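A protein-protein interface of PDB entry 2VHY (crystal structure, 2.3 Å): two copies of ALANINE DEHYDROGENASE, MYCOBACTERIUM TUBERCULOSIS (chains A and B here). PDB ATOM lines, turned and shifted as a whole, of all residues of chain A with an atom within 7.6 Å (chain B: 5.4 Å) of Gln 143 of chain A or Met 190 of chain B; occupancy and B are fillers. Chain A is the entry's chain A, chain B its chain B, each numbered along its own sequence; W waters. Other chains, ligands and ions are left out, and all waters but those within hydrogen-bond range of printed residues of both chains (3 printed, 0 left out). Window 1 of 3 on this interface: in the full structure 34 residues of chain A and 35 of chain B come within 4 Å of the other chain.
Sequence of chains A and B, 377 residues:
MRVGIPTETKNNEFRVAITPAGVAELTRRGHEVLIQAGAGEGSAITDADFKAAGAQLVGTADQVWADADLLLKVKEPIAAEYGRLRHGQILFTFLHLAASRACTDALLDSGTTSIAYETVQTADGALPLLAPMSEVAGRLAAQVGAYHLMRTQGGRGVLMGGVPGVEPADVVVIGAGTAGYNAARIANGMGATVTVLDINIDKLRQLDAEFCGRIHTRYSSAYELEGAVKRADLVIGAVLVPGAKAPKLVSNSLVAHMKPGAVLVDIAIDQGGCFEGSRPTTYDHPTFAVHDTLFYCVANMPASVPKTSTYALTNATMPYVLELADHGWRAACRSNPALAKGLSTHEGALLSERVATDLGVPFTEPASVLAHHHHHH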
ATOM      1  N   VAL A 136     -39.970 -22.463   6.993  1.00  0.00           N
ATOM      2  CA  VAL A 136     -39.454 -21.915   8.246  1.00  0.00           C
ATOM      3  C   VAL A 136     -38.858 -23.038   9.053  1.00  0.00           C
ATOM      4  O   VAL A 136     -37.715 -22.946   9.482  1.00  0.00           O
ATOM      5  CB  VAL A 136     -40.549 -21.227   9.111  1.00  0.00           C
ATOM      6  CG1 VAL A 136     -39.931 -20.698  10.387  1.00  0.00           C
ATOM      7  CG2 VAL A 136     -41.189 -20.082   8.347  1.00  0.00           C
ATOM      8  N   ALA A 137     -39.638 -24.104   9.237  1.00  0.00           N
ATOM      9  CA  ALA A 137     -39.213 -25.267  10.010  1.00  0.00           C
ATOM     10  C   ALA A 137     -37.883 -25.845   9.520  1.00  0.00           C
ATOM     11  O   ALA A 137     -37.084 -26.344  10.319  1.00  0.00           O
ATOM     12  CB  ALA A 137     -40.304 -26.333   9.975  1.00  0.00           C
ATOM     13  N   GLY A 138     -37.646 -25.769   8.212  1.00  0.00           N
ATOM     14  CA  GLY A 138     -36.414 -26.285   7.646  1.00  0.00           C
ATOM     15  C   GLY A 138     -35.194 -25.425   7.943  1.00  0.00           C
ATOM     16  O   GLY A 138     -34.095 -25.931   8.256  1.00  0.00           O
ATOM     17  N   ARG A 139     -35.380 -24.111   7.841  1.00  0.00           N
ATOM     18  CA  ARG A 139     -34.297 -23.171   8.102  1.00  0.00           C
ATOM     19  C   ARG A 139     -33.953 -23.097   9.588  1.00  0.00           C
ATOM     20  O   ARG A 139     -32.786 -22.965   9.954  1.00  0.00           O
ATOM     21  CB  ARG A 139     -34.685 -21.800   7.567  1.00  0.00           C
ATOM     22  CG  ARG A 139     -35.127 -21.868   6.128  1.00  0.00           C
ATOM     23  CD  ARG A 139     -35.023 -20.523   5.456  1.00  0.00           C
ATOM     24  NE  ARG A 139     -35.413 -20.607   4.055  1.00  0.00           N
ATOM     25  CZ  ARG A 139     -35.362 -19.588   3.208  1.00  0.00           C
ATOM     26  NH1 ARG A 139     -34.933 -18.402   3.623  1.00  0.00           N
ATOM     27  NH2 ARG A 139     -35.752 -19.760   1.952  1.00  0.00           N
ATOM     28  N   LEU A 140     -34.978 -23.192  10.431  1.00  0.00           N
ATOM     29  CA  LEU A 140     -34.832 -23.174  11.884  1.00  0.00           C
ATOM     30  C   LEU A 140     -34.005 -24.339  12.412  1.00  0.00           C
ATOM     31  O   LEU A 140     -33.184 -24.157  13.309  1.00  0.00           O
ATOM     32  CB  LEU A 140     -36.205 -23.221  12.541  1.00  0.00           C
ATOM     33  CG  LEU A 140     -36.708 -21.939  13.189  1.00  0.00           C
ATOM     34  CD1 LEU A 140     -38.142 -22.161  13.680  1.00  0.00           C
ATOM     35  CD2 LEU A 140     -35.774 -21.540  14.334  1.00  0.00           C
ATOM     36  N   ALA A 141     -34.246 -25.528  11.857  1.00  0.00           N
ATOM     37  CA  ALA A 141     -33.559 -26.759  12.236  1.00  0.00           C
ATOM     38  C   ALA A 141     -32.052 -26.599  12.176  1.00  0.00           C
ATOM     39  O   ALA A 141     -31.330 -27.054  13.067  1.00  0.00           O
ATOM     40  CB  ALA A 141     -33.996 -27.888  11.314  1.00  0.00           C
ATOM     41  N   ALA A 142     -31.584 -25.946  11.115  1.00  0.00           N
ATOM     42  CA  ALA A 142     -30.159 -25.703  10.910  1.00  0.00           C
ATOM     43  C   ALA A 142     -29.612 -24.677  11.897  1.00  0.00           C
ATOM     44  O   ALA A 142     -28.541 -24.886  12.470  1.00  0.00           O
ATOM     45  CB  ALA A 142     -29.905 -25.234   9.468  1.00  0.00           C
ATOM     46  N   GLN A 143     -30.340 -23.571  12.082  1.00  0.00           N
ATOM     47  CA  GLN A 143     -29.937 -22.508  13.017  1.00  0.00           C
ATOM     48  C   GLN A 143     -29.854 -23.082  14.421  1.00  0.00           C
ATOM     49  O   GLN A 143     -28.957 -22.743  15.192  1.00  0.00           O
ATOM     50  CB  GLN A 143     -30.946 -21.354  13.008  1.00  0.00           C
ATOM     51  CG  GLN A 143     -31.124 -20.715  11.641  1.00  0.00           C
ATOM     52  CD  GLN A 143     -31.887 -19.394  11.668  1.00  0.00           C
ATOM     53  OE1 GLN A 143     -32.026 -18.730  10.637  1.00  0.00           O
ATOM     54  NE2 GLN A 143     -32.384 -19.007  12.843  1.00  0.00           N
ATOM     55  N   VAL A 144     -30.818 -23.943  14.735  1.00  0.00           N
ATOM     56  CA  VAL A 144     -30.908 -24.624  16.019  1.00  0.00           C
ATOM     57  C   VAL A 144     -29.849 -25.732  16.139  1.00  0.00           C
ATOM     58  O   VAL A 144     -29.133 -25.810  17.143  1.00  0.00           O
ATOM     59  CB  VAL A 144     -32.314 -25.223  16.196  1.00  0.00           C
ATOM     60  CG1 VAL A 144     -32.292 -26.327  17.241  1.00  0.00           C
ATOM     61  CG2 VAL A 144     -33.288 -24.118  16.586  1.00  0.00           C
ATOM     62  N   GLY A 145     -29.746 -26.582  15.119  1.00  0.00           N
ATOM     63  CA  GLY A 145     -28.753 -27.640  15.151  1.00  0.00           C
ATOM     64  C   GLY A 145     -27.341 -27.088  15.265  1.00  0.00           C
ATOM     65  O   GLY A 145     -26.449 -27.716  15.847  1.00  0.00           O
ATOM     66  N   ALA A 146     -27.121 -25.914  14.689  1.00  0.00           N
ATOM     67  CA  ALA A 146     -25.809 -25.279  14.740  1.00  0.00           C
ATOM     68  C   ALA A 146     -25.554 -24.756  16.152  1.00  0.00           C
ATOM     69  O   ALA A 146     -24.408 -24.638  16.599  1.00  0.00           O
ATOM     70  CB  ALA A 146     -25.749 -24.130  13.748  1.00  0.00           C
ATOM     71  N   TYR A 147     -26.642 -24.446  16.848  1.00  0.00           N
ATOM     72  CA  TYR A 147     -26.563 -23.916  18.189  1.00  0.00           C
ATOM     73  C   TYR A 147     -26.344 -24.982  19.243  1.00  0.00           C
ATOM     74  O   TYR A 147     -25.508 -24.832  20.129  1.00  0.00           O
ATOM     75  CB  TYR A 147     -27.828 -23.143  18.524  1.00  0.00           C
ATOM     76  CG  TYR A 147     -27.651 -22.320  19.766  1.00  0.00           C
ATOM     77  CD1 TYR A 147     -28.144 -22.749  20.993  1.00  0.00           C
ATOM     78  CD2 TYR A 147     -26.925 -21.133  19.722  1.00  0.00           C
ATOM     79  CE1 TYR A 147     -27.911 -22.013  22.144  1.00  0.00           C
ATOM     80  CE2 TYR A 147     -26.688 -20.396  20.861  1.00  0.00           C
ATOM     81  CZ  TYR A 147     -27.179 -20.837  22.066  1.00  0.00           C
ATOM     82  OH  TYR A 147     -26.920 -20.092  23.188  1.00  0.00           O
ATOM     83  N   HIS A 148     -27.103 -26.062  19.163  1.00  0.00           N
ATOM     84  CA  HIS A 148     -26.936 -27.118  20.136  1.00  0.00           C
ATOM     85  C   HIS A 148     -25.689 -27.965  19.899  1.00  0.00           C
ATOM     86  O   HIS A 148     -25.391 -28.866  20.683  1.00  0.00           O
ATOM     87  CB  HIS A 148     -28.202 -27.960  20.186  1.00  0.00           C
ATOM     88  CG  HIS A 148     -29.370 -27.212  20.741  1.00  0.00           C
ATOM     89  ND1 HIS A 148     -30.420 -27.829  21.382  1.00  0.00           N
ATOM     90  CD2 HIS A 148     -29.621 -25.883  20.802  1.00  0.00           C
ATOM     91  CE1 HIS A 148     -31.264 -26.912  21.820  1.00  0.00           C
ATOM     92  NE2 HIS A 148     -30.802 -25.723  21.480  1.00  0.00           N
ATOM     93  N   LEU A 149     -24.950 -27.650  18.833  1.00  0.00           N
ATOM     94  CA  LEU A 149     -23.711 -28.352  18.488  1.00  0.00           C
ATOM     95  C   LEU A 149     -22.581 -27.857  19.388  1.00  0.00           C
ATOM     96  O   LEU A 149     -21.514 -28.464  19.457  1.00  0.00           O
ATOM     97  CB  LEU A 149     -23.326 -28.092  17.024  1.00  0.00           C
ATOM     98  CG  LEU A 149     -23.386 -29.196  15.961  1.00  0.00           C
ATOM     99  CD1 LEU A 149     -22.777 -28.677  14.651  1.00  0.00           C
ATOM    100  CD2 LEU A 149     -22.627 -30.418  16.450  1.00  0.00           C
ATOM    101  N   MET A 160     -20.073 -24.704  12.737  1.00  0.00           N
ATOM    102  CA  MET A 160     -20.668 -25.136  11.479  1.00  0.00           C
ATOM    103  C   MET A 160     -19.733 -25.121  10.278  1.00  0.00           C
ATOM    104  O   MET A 160     -19.609 -26.116   9.576  1.00  0.00           O
ATOM    105  CB  MET A 160     -21.894 -24.272  11.152  1.00  0.00           C
ATOM    106  CG  MET A 160     -23.125 -24.593  11.972  1.00  0.00           C
ATOM    107  SD  MET A 160     -23.729 -26.254  11.637  1.00  0.00           S
ATOM    108  CE  MET A 160     -24.873 -25.938  10.297  1.00  0.00           C
ATOM    109  N   ALA A 183     -33.076 -26.744   5.183  1.00  0.00           N
ATOM    110  CA  ALA A 183     -32.042 -27.021   6.165  1.00  0.00           C
ATOM    111  C   ALA A 183     -30.671 -27.051   5.468  1.00  0.00           C
ATOM    112  O   ALA A 183     -29.732 -26.394   5.922  1.00  0.00           O
ATOM    113  CB  ALA A 183     -32.339 -28.358   6.875  1.00  0.00           C
ATOM    114  N   ARG A 185     -29.817 -25.739   2.670  1.00  0.00           N
ATOM    115  CA  ARG A 185     -29.570 -24.386   2.189  1.00  0.00           C
ATOM    116  C   ARG A 185     -28.852 -23.595   3.260  1.00  0.00           C
ATOM    117  O   ARG A 185     -27.752 -23.095   3.031  1.00  0.00           O
ATOM    118  CB  ARG A 185     -30.901 -23.709   1.839  1.00  0.00           C
ATOM    119  CG  ARG A 185     -30.880 -22.185   1.859  1.00  0.00           C
ATOM    120  CD  ARG A 185     -30.621 -21.560   0.493  1.00  0.00           C
ATOM    121  NE  ARG A 185     -31.849 -21.374  -0.290  1.00  0.00           N
ATOM    122  CZ  ARG A 185     -32.429 -20.196  -0.522  1.00  0.00           C
ATOM    123  NH1 ARG A 185     -31.903 -19.075  -0.032  1.00  0.00           N
ATOM    124  NH2 ARG A 185     -33.526 -20.139  -1.265  1.00  0.00           N
ATOM    125  N   ILE A 186     -29.468 -23.506   4.437  1.00  0.00           N
ATOM    126  CA  ILE A 186     -28.907 -22.747   5.567  1.00  0.00           C
ATOM    127  C   ILE A 186     -27.661 -23.373   6.163  1.00  0.00           C
ATOM    128  O   ILE A 186     -26.686 -22.683   6.436  1.00  0.00           O
ATOM    129  CB  ILE A 186     -29.961 -22.539   6.695  1.00  0.00           C
ATOM    130  CG1 ILE A 186     -31.159 -21.771   6.144  1.00  0.00           C
ATOM    131  CG2 ILE A 186     -29.368 -21.741   7.839  1.00  0.00           C
ATOM    132  CD1 ILE A 186     -30.781 -20.527   5.352  1.00  0.00           C
ATOM    133  N   ALA A 187     -27.694 -24.680   6.373  1.00  0.00           N
ATOM    134  CA  ALA A 187     -26.534 -25.373   6.906  1.00  0.00           C
ATOM    135  C   ALA A 187     -25.333 -25.139   5.967  1.00  0.00           C
ATOM    136  O   ALA A 187     -24.198 -25.018   6.417  1.00  0.00           O
ATOM    137  CB  ALA A 187     -26.845 -26.875   7.035  1.00  0.00           C
ATOM    138  N   ASN A 188     -25.596 -25.074   4.664  1.00  0.00           N
ATOM    139  CA  ASN A 188     -24.548 -24.853   3.665  1.00  0.00           C
ATOM    140  C   ASN A 188     -24.033 -23.400   3.748  1.00  0.00           C
ATOM    141  O   ASN A 188     -22.833 -23.129   3.603  1.00  0.00           O
ATOM    142  CB  ASN A 188     -25.107 -25.154   2.265  1.00  0.00           C
ATOM    143  CG  ASN A 188     -24.026 -25.206   1.190  1.00  0.00           C
ATOM    144  OD1 ASN A 188     -23.097 -26.005   1.269  1.00  0.00           O
ATOM    145  ND2 ASN A 188     -24.155 -24.363   0.177  1.00  0.00           N
ATOM    146  N   GLY A 189     -24.948 -22.466   3.991  1.00  0.00           N
ATOM    147  CA  GLY A 189     -24.554 -21.076   4.095  1.00  0.00           C
ATOM    148  C   GLY A 189     -23.713 -20.803   5.326  1.00  0.00           C
ATOM    149  O   GLY A 189     -22.997 -19.806   5.394  1.00  0.00           O
ATOM    150  N   MET A 190     -23.802 -21.685   6.311  1.00  0.00           N
ATOM    151  CA  MET A 190     -23.029 -21.517   7.533  1.00  0.00           C
ATOM    152  C   MET A 190     -21.636 -22.075   7.378  1.00  0.00           C
ATOM    153  O   MET A 190     -20.859 -22.097   8.333  1.00  0.00           O
ATOM    154  CB  MET A 190     -23.739 -22.172   8.702  1.00  0.00           C
ATOM    155  CG  MET A 190     -25.030 -21.474   8.975  1.00  0.00           C
ATOM    156  SD  MET A 190     -25.986 -22.162  10.275  1.00  0.00           S
ATOM    157  CE  MET A 190     -25.129 -21.442  11.686  1.00  0.00           C
ATOM    158  N   GLY A 191     -21.330 -22.516   6.158  1.00  0.00           N
ATOM    159  CA  GLY A 191     -20.015 -23.043   5.856  1.00  0.00           C
ATOM    160  C   GLY A 191     -19.900 -24.537   5.983  1.00  0.00           C
ATOM    161  O   GLY A 191     -18.926 -25.118   5.531  1.00  0.00           O
ATOM    162  N   LEU A 234     -24.124 -33.108  12.788  1.00  0.00           N
ATOM    163  CA  LEU A 234     -25.521 -32.709  12.902  1.00  0.00           C
ATOM    164  C   LEU A 234     -26.330 -33.432  11.821  1.00  0.00           C
ATOM    165  O   LEU A 234     -25.990 -33.340  10.635  1.00  0.00           O
ATOM    166  CB  LEU A 234     -25.665 -31.196  12.673  1.00  0.00           C
ATOM    167  CG  LEU A 234     -26.892 -30.399  13.164  1.00  0.00           C
ATOM    168  CD1 LEU A 234     -27.230 -29.334  12.120  1.00  0.00           C
ATOM    169  CD2 LEU A 234     -28.101 -31.301  13.417  1.00  0.00           C
ATOM    170  N   ILE A 236     -30.231 -33.827  10.331  1.00  0.00           N
ATOM    171  CA  ILE A 236     -31.544 -33.191  10.345  1.00  0.00           C
ATOM    172  C   ILE A 236     -32.615 -34.089   9.719  1.00  0.00           C
ATOM    173  O   ILE A 236     -32.551 -34.392   8.539  1.00  0.00           O
ATOM    174  CB  ILE A 236     -31.499 -31.836   9.577  1.00  0.00           C
ATOM    175  CG1 ILE A 236     -30.404 -30.942  10.164  1.00  0.00           C
ATOM    176  CG2 ILE A 236     -32.845 -31.125   9.667  1.00  0.00           C
ATOM    177  CD1 ILE A 236     -30.321 -29.574   9.539  1.00  0.00           C
ATOM    178  N   VAL A 265     -31.583 -33.330  14.887  1.00  0.00           N
ATOM    179  CA  VAL A 265     -32.769 -32.513  15.014  1.00  0.00           C
ATOM    180  C   VAL A 265     -33.800 -33.256  14.201  1.00  0.00           C
ATOM    181  O   VAL A 265     -33.525 -33.664  13.081  1.00  0.00           O
ATOM    182  CB  VAL A 265     -32.585 -31.118  14.392  1.00  0.00           C
ATOM    183  CG1 VAL A 265     -33.726 -30.199  14.837  1.00  0.00           C
ATOM    184  CG2 VAL A 265     -31.230 -30.544  14.770  1.00  0.00           C
ATOM    185  N   VAL A 305     -40.245 -18.166  15.670  1.00  0.00           N
ATOM    186  CA  VAL A 305     -39.944 -16.921  14.968  1.00  0.00           C
ATOM    187  C   VAL A 305     -41.274 -16.392  14.427  1.00  0.00           C
ATOM    188  O   VAL A 305     -41.493 -16.364  13.216  1.00  0.00           O
ATOM    189  CB  VAL A 305     -38.933 -17.143  13.797  1.00  0.00           C
ATOM    190  CG1 VAL A 305     -37.562 -17.465  14.350  1.00  0.00           C
ATOM    191  CG2 VAL A 305     -39.399 -18.263  12.895  1.00  0.00           C
ATOM    192  N   ALA B 142     -22.622 -14.741  15.068  1.00  0.00           N
ATOM    193  CA  ALA B 142     -23.744 -14.880  14.132  1.00  0.00           C
ATOM    194  C   ALA B 142     -24.665 -16.059  14.425  1.00  0.00           C
ATOM    195  O   ALA B 142     -25.884 -15.927  14.362  1.00  0.00           O
ATOM    196  CB  ALA B 142     -23.213 -14.978  12.690  1.00  0.00           C
ATOM    197  N   GLN B 143     -24.077 -17.213  14.721  1.00  0.00           N
ATOM    198  CA  GLN B 143     -24.847 -18.409  15.017  1.00  0.00           C
ATOM    199  C   GLN B 143     -25.567 -18.212  16.326  1.00  0.00           C
ATOM    200  O   GLN B 143     -26.684 -18.671  16.497  1.00  0.00           O
ATOM    201  CB  GLN B 143     -23.931 -19.633  15.131  1.00  0.00           C
ATOM    202  CG  GLN B 143     -22.919 -19.754  13.996  1.00  0.00           C
ATOM    203  CD  GLN B 143     -22.405 -21.168  13.793  1.00  0.00           C
ATOM    204  OE1 GLN B 143     -22.053 -21.861  14.748  1.00  0.00           O
ATOM    205  NE2 GLN B 143     -22.349 -21.597  12.533  1.00  0.00           N
ATOM    206  N   ALA B 146     -28.250 -15.375  15.867  1.00  0.00           N
ATOM    207  CA  ALA B 146     -29.398 -15.876  15.117  1.00  0.00           C
ATOM    208  C   ALA B 146     -30.346 -16.691  15.986  1.00  0.00           C
ATOM    209  O   ALA B 146     -31.566 -16.630  15.814  1.00  0.00           O
ATOM    210  CB  ALA B 146     -28.925 -16.720  13.964  1.00  0.00           C
ATOM    211  N   TYR B 147     -29.777 -17.467  16.905  1.00  0.00           N
ATOM    212  CA  TYR B 147     -30.554 -18.299  17.822  1.00  0.00           C
ATOM    213  C   TYR B 147     -31.286 -17.434  18.840  1.00  0.00           C
ATOM    214  O   TYR B 147     -32.472 -17.633  19.093  1.00  0.00           O
ATOM    215  CB  TYR B 147     -29.631 -19.280  18.551  1.00  0.00           C
ATOM    216  CG  TYR B 147     -30.343 -20.256  19.467  1.00  0.00           C
ATOM    217  CD1 TYR B 147     -30.667 -19.916  20.778  1.00  0.00           C
ATOM    218  CD2 TYR B 147     -30.700 -21.525  19.008  1.00  0.00           C
ATOM    219  CE1 TYR B 147     -31.332 -20.826  21.616  1.00  0.00           C
ATOM    220  CE2 TYR B 147     -31.364 -22.438  19.831  1.00  0.00           C
ATOM    221  CZ  TYR B 147     -31.680 -22.087  21.135  1.00  0.00           C
ATOM    222  OH  TYR B 147     -32.351 -22.997  21.931  1.00  0.00           O
ATOM    223  N   LEU B 159     -36.600 -14.841  11.767  1.00  0.00           N
ATOM    224  CA  LEU B 159     -35.702 -15.849  11.210  1.00  0.00           C
ATOM    225  C   LEU B 159     -34.627 -15.147  10.361  1.00  0.00           C
ATOM    226  O   LEU B 159     -34.964 -14.346   9.495  1.00  0.00           O
ATOM    227  CB  LEU B 159     -36.504 -16.819  10.341  1.00  0.00           C
ATOM    228  CG  LEU B 159     -35.742 -17.952   9.658  1.00  0.00           C
ATOM    229  CD1 LEU B 159     -35.255 -18.940  10.707  1.00  0.00           C
ATOM    230  CD2 LEU B 159     -36.644 -18.635   8.645  1.00  0.00           C
ATOM    231  N   MET B 160     -33.354 -15.454  10.614  1.00  0.00           N
ATOM    232  CA  MET B 160     -32.225 -14.854   9.893  1.00  0.00           C
ATOM    233  C   MET B 160     -32.419 -14.571   8.411  1.00  0.00           C
ATOM    234  O   MET B 160     -32.036 -13.512   7.928  1.00  0.00           O
ATOM    235  CB  MET B 160     -30.973 -15.716  10.038  1.00  0.00           C
ATOM    236  CG  MET B 160     -30.242 -15.561  11.346  1.00  0.00           C
ATOM    237  SD  MET B 160     -29.440 -13.971  11.536  1.00  0.00           S
ATOM    238  CE  MET B 160     -27.714 -14.355  11.239  1.00  0.00           C
ATOM    239  N   GLY B 161     -32.989 -15.513   7.673  1.00  0.00           N
ATOM    240  CA  GLY B 161     -33.171 -15.269   6.258  1.00  0.00           C
ATOM    241  C   GLY B 161     -34.604 -15.267   5.779  1.00  0.00           C
ATOM    242  O   GLY B 161     -34.836 -15.362   4.576  1.00  0.00           O
ATOM    243  N   ARG B 185     -19.975 -12.734   7.042  1.00  0.00           N
ATOM    244  CA  ARG B 185     -19.953 -13.910   6.179  1.00  0.00           C
ATOM    245  C   ARG B 185     -21.054 -14.890   6.593  1.00  0.00           C
ATOM    246  O   ARG B 185     -21.934 -15.200   5.799  1.00  0.00           O
ATOM    247  CB  ARG B 185     -18.577 -14.603   6.249  1.00  0.00           C
ATOM    248  CG  ARG B 185     -18.559 -16.062   5.770  1.00  0.00           C
ATOM    249  CD  ARG B 185     -18.235 -16.193   4.298  1.00  0.00           C
ATOM    250  NE  ARG B 185     -16.802 -16.372   4.074  1.00  0.00           N
ATOM    251  CZ  ARG B 185     -16.180 -17.552   4.018  1.00  0.00           C
ATOM    252  NH1 ARG B 185     -16.854 -18.684   4.167  1.00  0.00           N
ATOM    253  NH2 ARG B 185     -14.872 -17.596   3.817  1.00  0.00           N
ATOM    254  N   ILE B 186     -21.027 -15.364   7.834  1.00  0.00           N
ATOM    255  CA  ILE B 186     -22.041 -16.327   8.282  1.00  0.00           C
ATOM    256  C   ILE B 186     -23.476 -15.774   8.282  1.00  0.00           C
ATOM    257  O   ILE B 186     -24.372 -16.418   7.737  1.00  0.00           O
ATOM    258  CB  ILE B 186     -21.703 -16.899   9.700  1.00  0.00           C
ATOM    259  CG1 ILE B 186     -20.298 -17.518   9.694  1.00  0.00           C
ATOM    260  CG2 ILE B 186     -22.728 -17.974  10.104  1.00  0.00           C
ATOM    261  CD1 ILE B 186     -20.173 -18.798   8.877  1.00  0.00           C
ATOM    262  N   ALA B 187     -23.699 -14.599   8.879  1.00  0.00           N
ATOM    263  CA  ALA B 187     -25.044 -14.012   8.915  1.00  0.00           C
ATOM    264  C   ALA B 187     -25.623 -13.941   7.505  1.00  0.00           C
ATOM    265  O   ALA B 187     -26.805 -14.213   7.292  1.00  0.00           O
ATOM    266  CB  ALA B 187     -24.995 -12.615   9.537  1.00  0.00           C
ATOM    267  N   ASN B 188     -24.770 -13.564   6.549  1.00  0.00           N
ATOM    268  CA  ASN B 188     -25.137 -13.453   5.132  1.00  0.00           C
ATOM    269  C   ASN B 188     -25.449 -14.811   4.545  1.00  0.00           C
ATOM    270  O   ASN B 188     -26.369 -14.952   3.748  1.00  0.00           O
ATOM    271  CB  ASN B 188     -23.986 -12.851   4.324  1.00  0.00           C
ATOM    272  CG  ASN B 188     -24.137 -13.076   2.806  1.00  0.00           C
ATOM    273  OD1 ASN B 188     -24.988 -12.471   2.174  1.00  0.00           O
ATOM    274  ND2 ASN B 188     -23.297 -13.952   2.231  1.00  0.00           N
ATOM    275  N   GLY B 189     -24.645 -15.799   4.916  1.00  0.00           N
ATOM    276  CA  GLY B 189     -24.851 -17.144   4.431  1.00  0.00           C
ATOM    277  C   GLY B 189     -26.117 -17.728   5.007  1.00  0.00           C
ATOM    278  O   GLY B 189     -26.749 -18.602   4.411  1.00  0.00           O
ATOM    279  N   MET B 190     -26.491 -17.256   6.188  1.00  0.00           N
ATOM    280  CA  MET B 190     -27.703 -17.736   6.831  1.00  0.00           C
ATOM    281  C   MET B 190     -28.914 -17.049   6.228  1.00  0.00           C
ATOM    282  O   MET B 190     -30.047 -17.409   6.523  1.00  0.00           O
ATOM    283  CB  MET B 190     -27.657 -17.464   8.329  1.00  0.00           C
ATOM    284  CG  MET B 190     -26.568 -18.197   9.034  1.00  0.00           C
ATOM    285  SD  MET B 190     -26.544 -17.691  10.726  1.00  0.00           S
ATOM    286  CE  MET B 190     -27.852 -18.668  11.355  1.00  0.00           C
ATOM    287  N   GLY B 191     -28.664 -16.033   5.407  1.00  0.00           N
ATOM    288  CA  GLY B 191     -29.745 -15.319   4.743  1.00  0.00           C
ATOM    289  C   GLY B 191     -30.096 -13.916   5.200  1.00  0.00           C
ATOM    290  O   GLY B 191     -30.907 -13.271   4.562  1.00  0.00           O
ATOM    291  N   ALA B 192     -29.506 -13.432   6.289  1.00  0.00           N
ATOM    292  CA  ALA B 192     -29.829 -12.088   6.773  1.00  0.00           C
ATOM    293  C   ALA B 192     -29.383 -11.007   5.794  1.00  0.00           C
ATOM    294  O   ALA B 192     -28.578 -11.265   4.903  1.00  0.00           O
ATOM    295  CB  ALA B 192     -29.172 -11.853   8.121  1.00  0.00           C
HETATM  296  O   HOH W   1     -32.845 -18.560   7.894  1.00  0.00           O
HETATM  297  O   HOH W   2     -22.020 -24.700  15.428  1.00  0.00           O
HETATM  298  O   HOH W   3     -20.003 -21.274  10.778  1.00  0.00           O
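Water W3 lies within hydrogen-bond range of O of Met 190 of chain A (2.7 Å) and NE2 of Gln 143 of chain B (2.9 Å). Water W1 lies within hydrogen-bond range of OE1 of Gln 143 of chain A (2.9 Å), N of Gly 161 of chain B (3.1 Å) and O of Met 190 of chain B (3.3 Å).
Gln 143 of chain A touches Met 190 of chain B, and with the chains exchanged Met 190 of chain A touches Gln 143 of chain B. Of the 15 pairs that touch across the chains among the printed residues, 9 have their exchanged pair printed and touching as well.
Of the 15 printed residues of chain B, 9 touch a printed residue of chain A. Printed residues of chain B that touch a printed residue of chain A: Gln 143, Ala 146, Tyr 147, Leu 159, Met 160, Gly 161, Ile 186, Gly 189 and Met 190. Hydrophobic or aromatic side chains of chain B within 4 Å of the printed part of chain A: Tyr 147, Leu 159, Met 160, Ile 186 and Met 190. Along chain B the printed residues that touch a printed residue of chain A span positions 143 to 190. Among the printed residues, no Asp or Glu carboxylate lies within 4 Å of a Lys or Arg side-chain nitrogen of the other chain.
NH1 of Arg 139 of chain A sits at hydrogen-bond distance from O of Gly 161 of chain B (3.2 Å). A ring nitrogen (NE2) of His 148 of chain A is in hydrogen-bond range of the side-chain hydroxyl (OH) of Tyr 147 of chain B, at 3.2 Å.
The backbone carbonyl oxygen (O) of Met 160 of chain B sits close to the backbone NH (N) of Ala 192 of chain B, 3.0 Å away.
Of chain B, only Ala 146 (3.9 Å), Leu 159 (3.2 Å), Met 160 (3.2 Å) and Met 190 (3.9 Å) come within 4 Å of Gln 143 of chain A. Of chain A, only Gln 143 (3.9 Å), Ile 186 (3.4 Å) and Met 190 (3.6 Å) come within 4 Å of Met 190 of chain B. Gly 189 of chain B touches just one residue of chain A: Gly 189. Printed residues of chain B within 4 Å of Met 160 of chain A: Gln 143. Printed residues of chain B within 4 Å of Ile 186 of chain A: Met 190. Ala 142 of chain A touches none of the printed residues of chain B. Ala 146 of chain A touches none of the printed residues of chain B. The nearest residue of chain B that does not touch Gln 143 of chain A is Tyr 147 of chain B (4.4 Å). The nearest residue of chain A that does not touch Met 190 of chain B is Gly 189 of chain A (4.4 Å). The nearest printed residue of chain A that does not touch Gly 161 of chain B is Gln 143 of chain A (4.5 Å).
Among the printed residues, pairs that only touch across the chains: Met 190 of chain A with Gln 143 of chain B (2.9 Å), Met 160 of chain A with Gln 143 of chain B (3.0 Å), Gln 143 of chain A with Leu 159 of chain B (3.2 Å), Tyr 147 of chain A with Tyr 147 of chain B (3.2 Å), Gln 143 of chain A with Met 160 of chain B (3.2 Å), Gly 189 of chain A with Gly 189 of chain B (3.3 Å), Ile 186 of chain A with Met 190 of chain B (3.4 Å), Met 190 of chain A with Ile 186 of chain B (3.4 Å), Met 190 of chain A with Met 190 of chain B (3.6 Å), Val 305 of chain A with Leu 159 of chain B (3.8 Å), Gln 143 of chain A with Met 190 of chain B (3.9 Å), Arg 139 of chain A with Leu 159 of chain B (3.9 Å) and Gln 143 of chain A with Ala 146 of chain B (3.9 Å).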
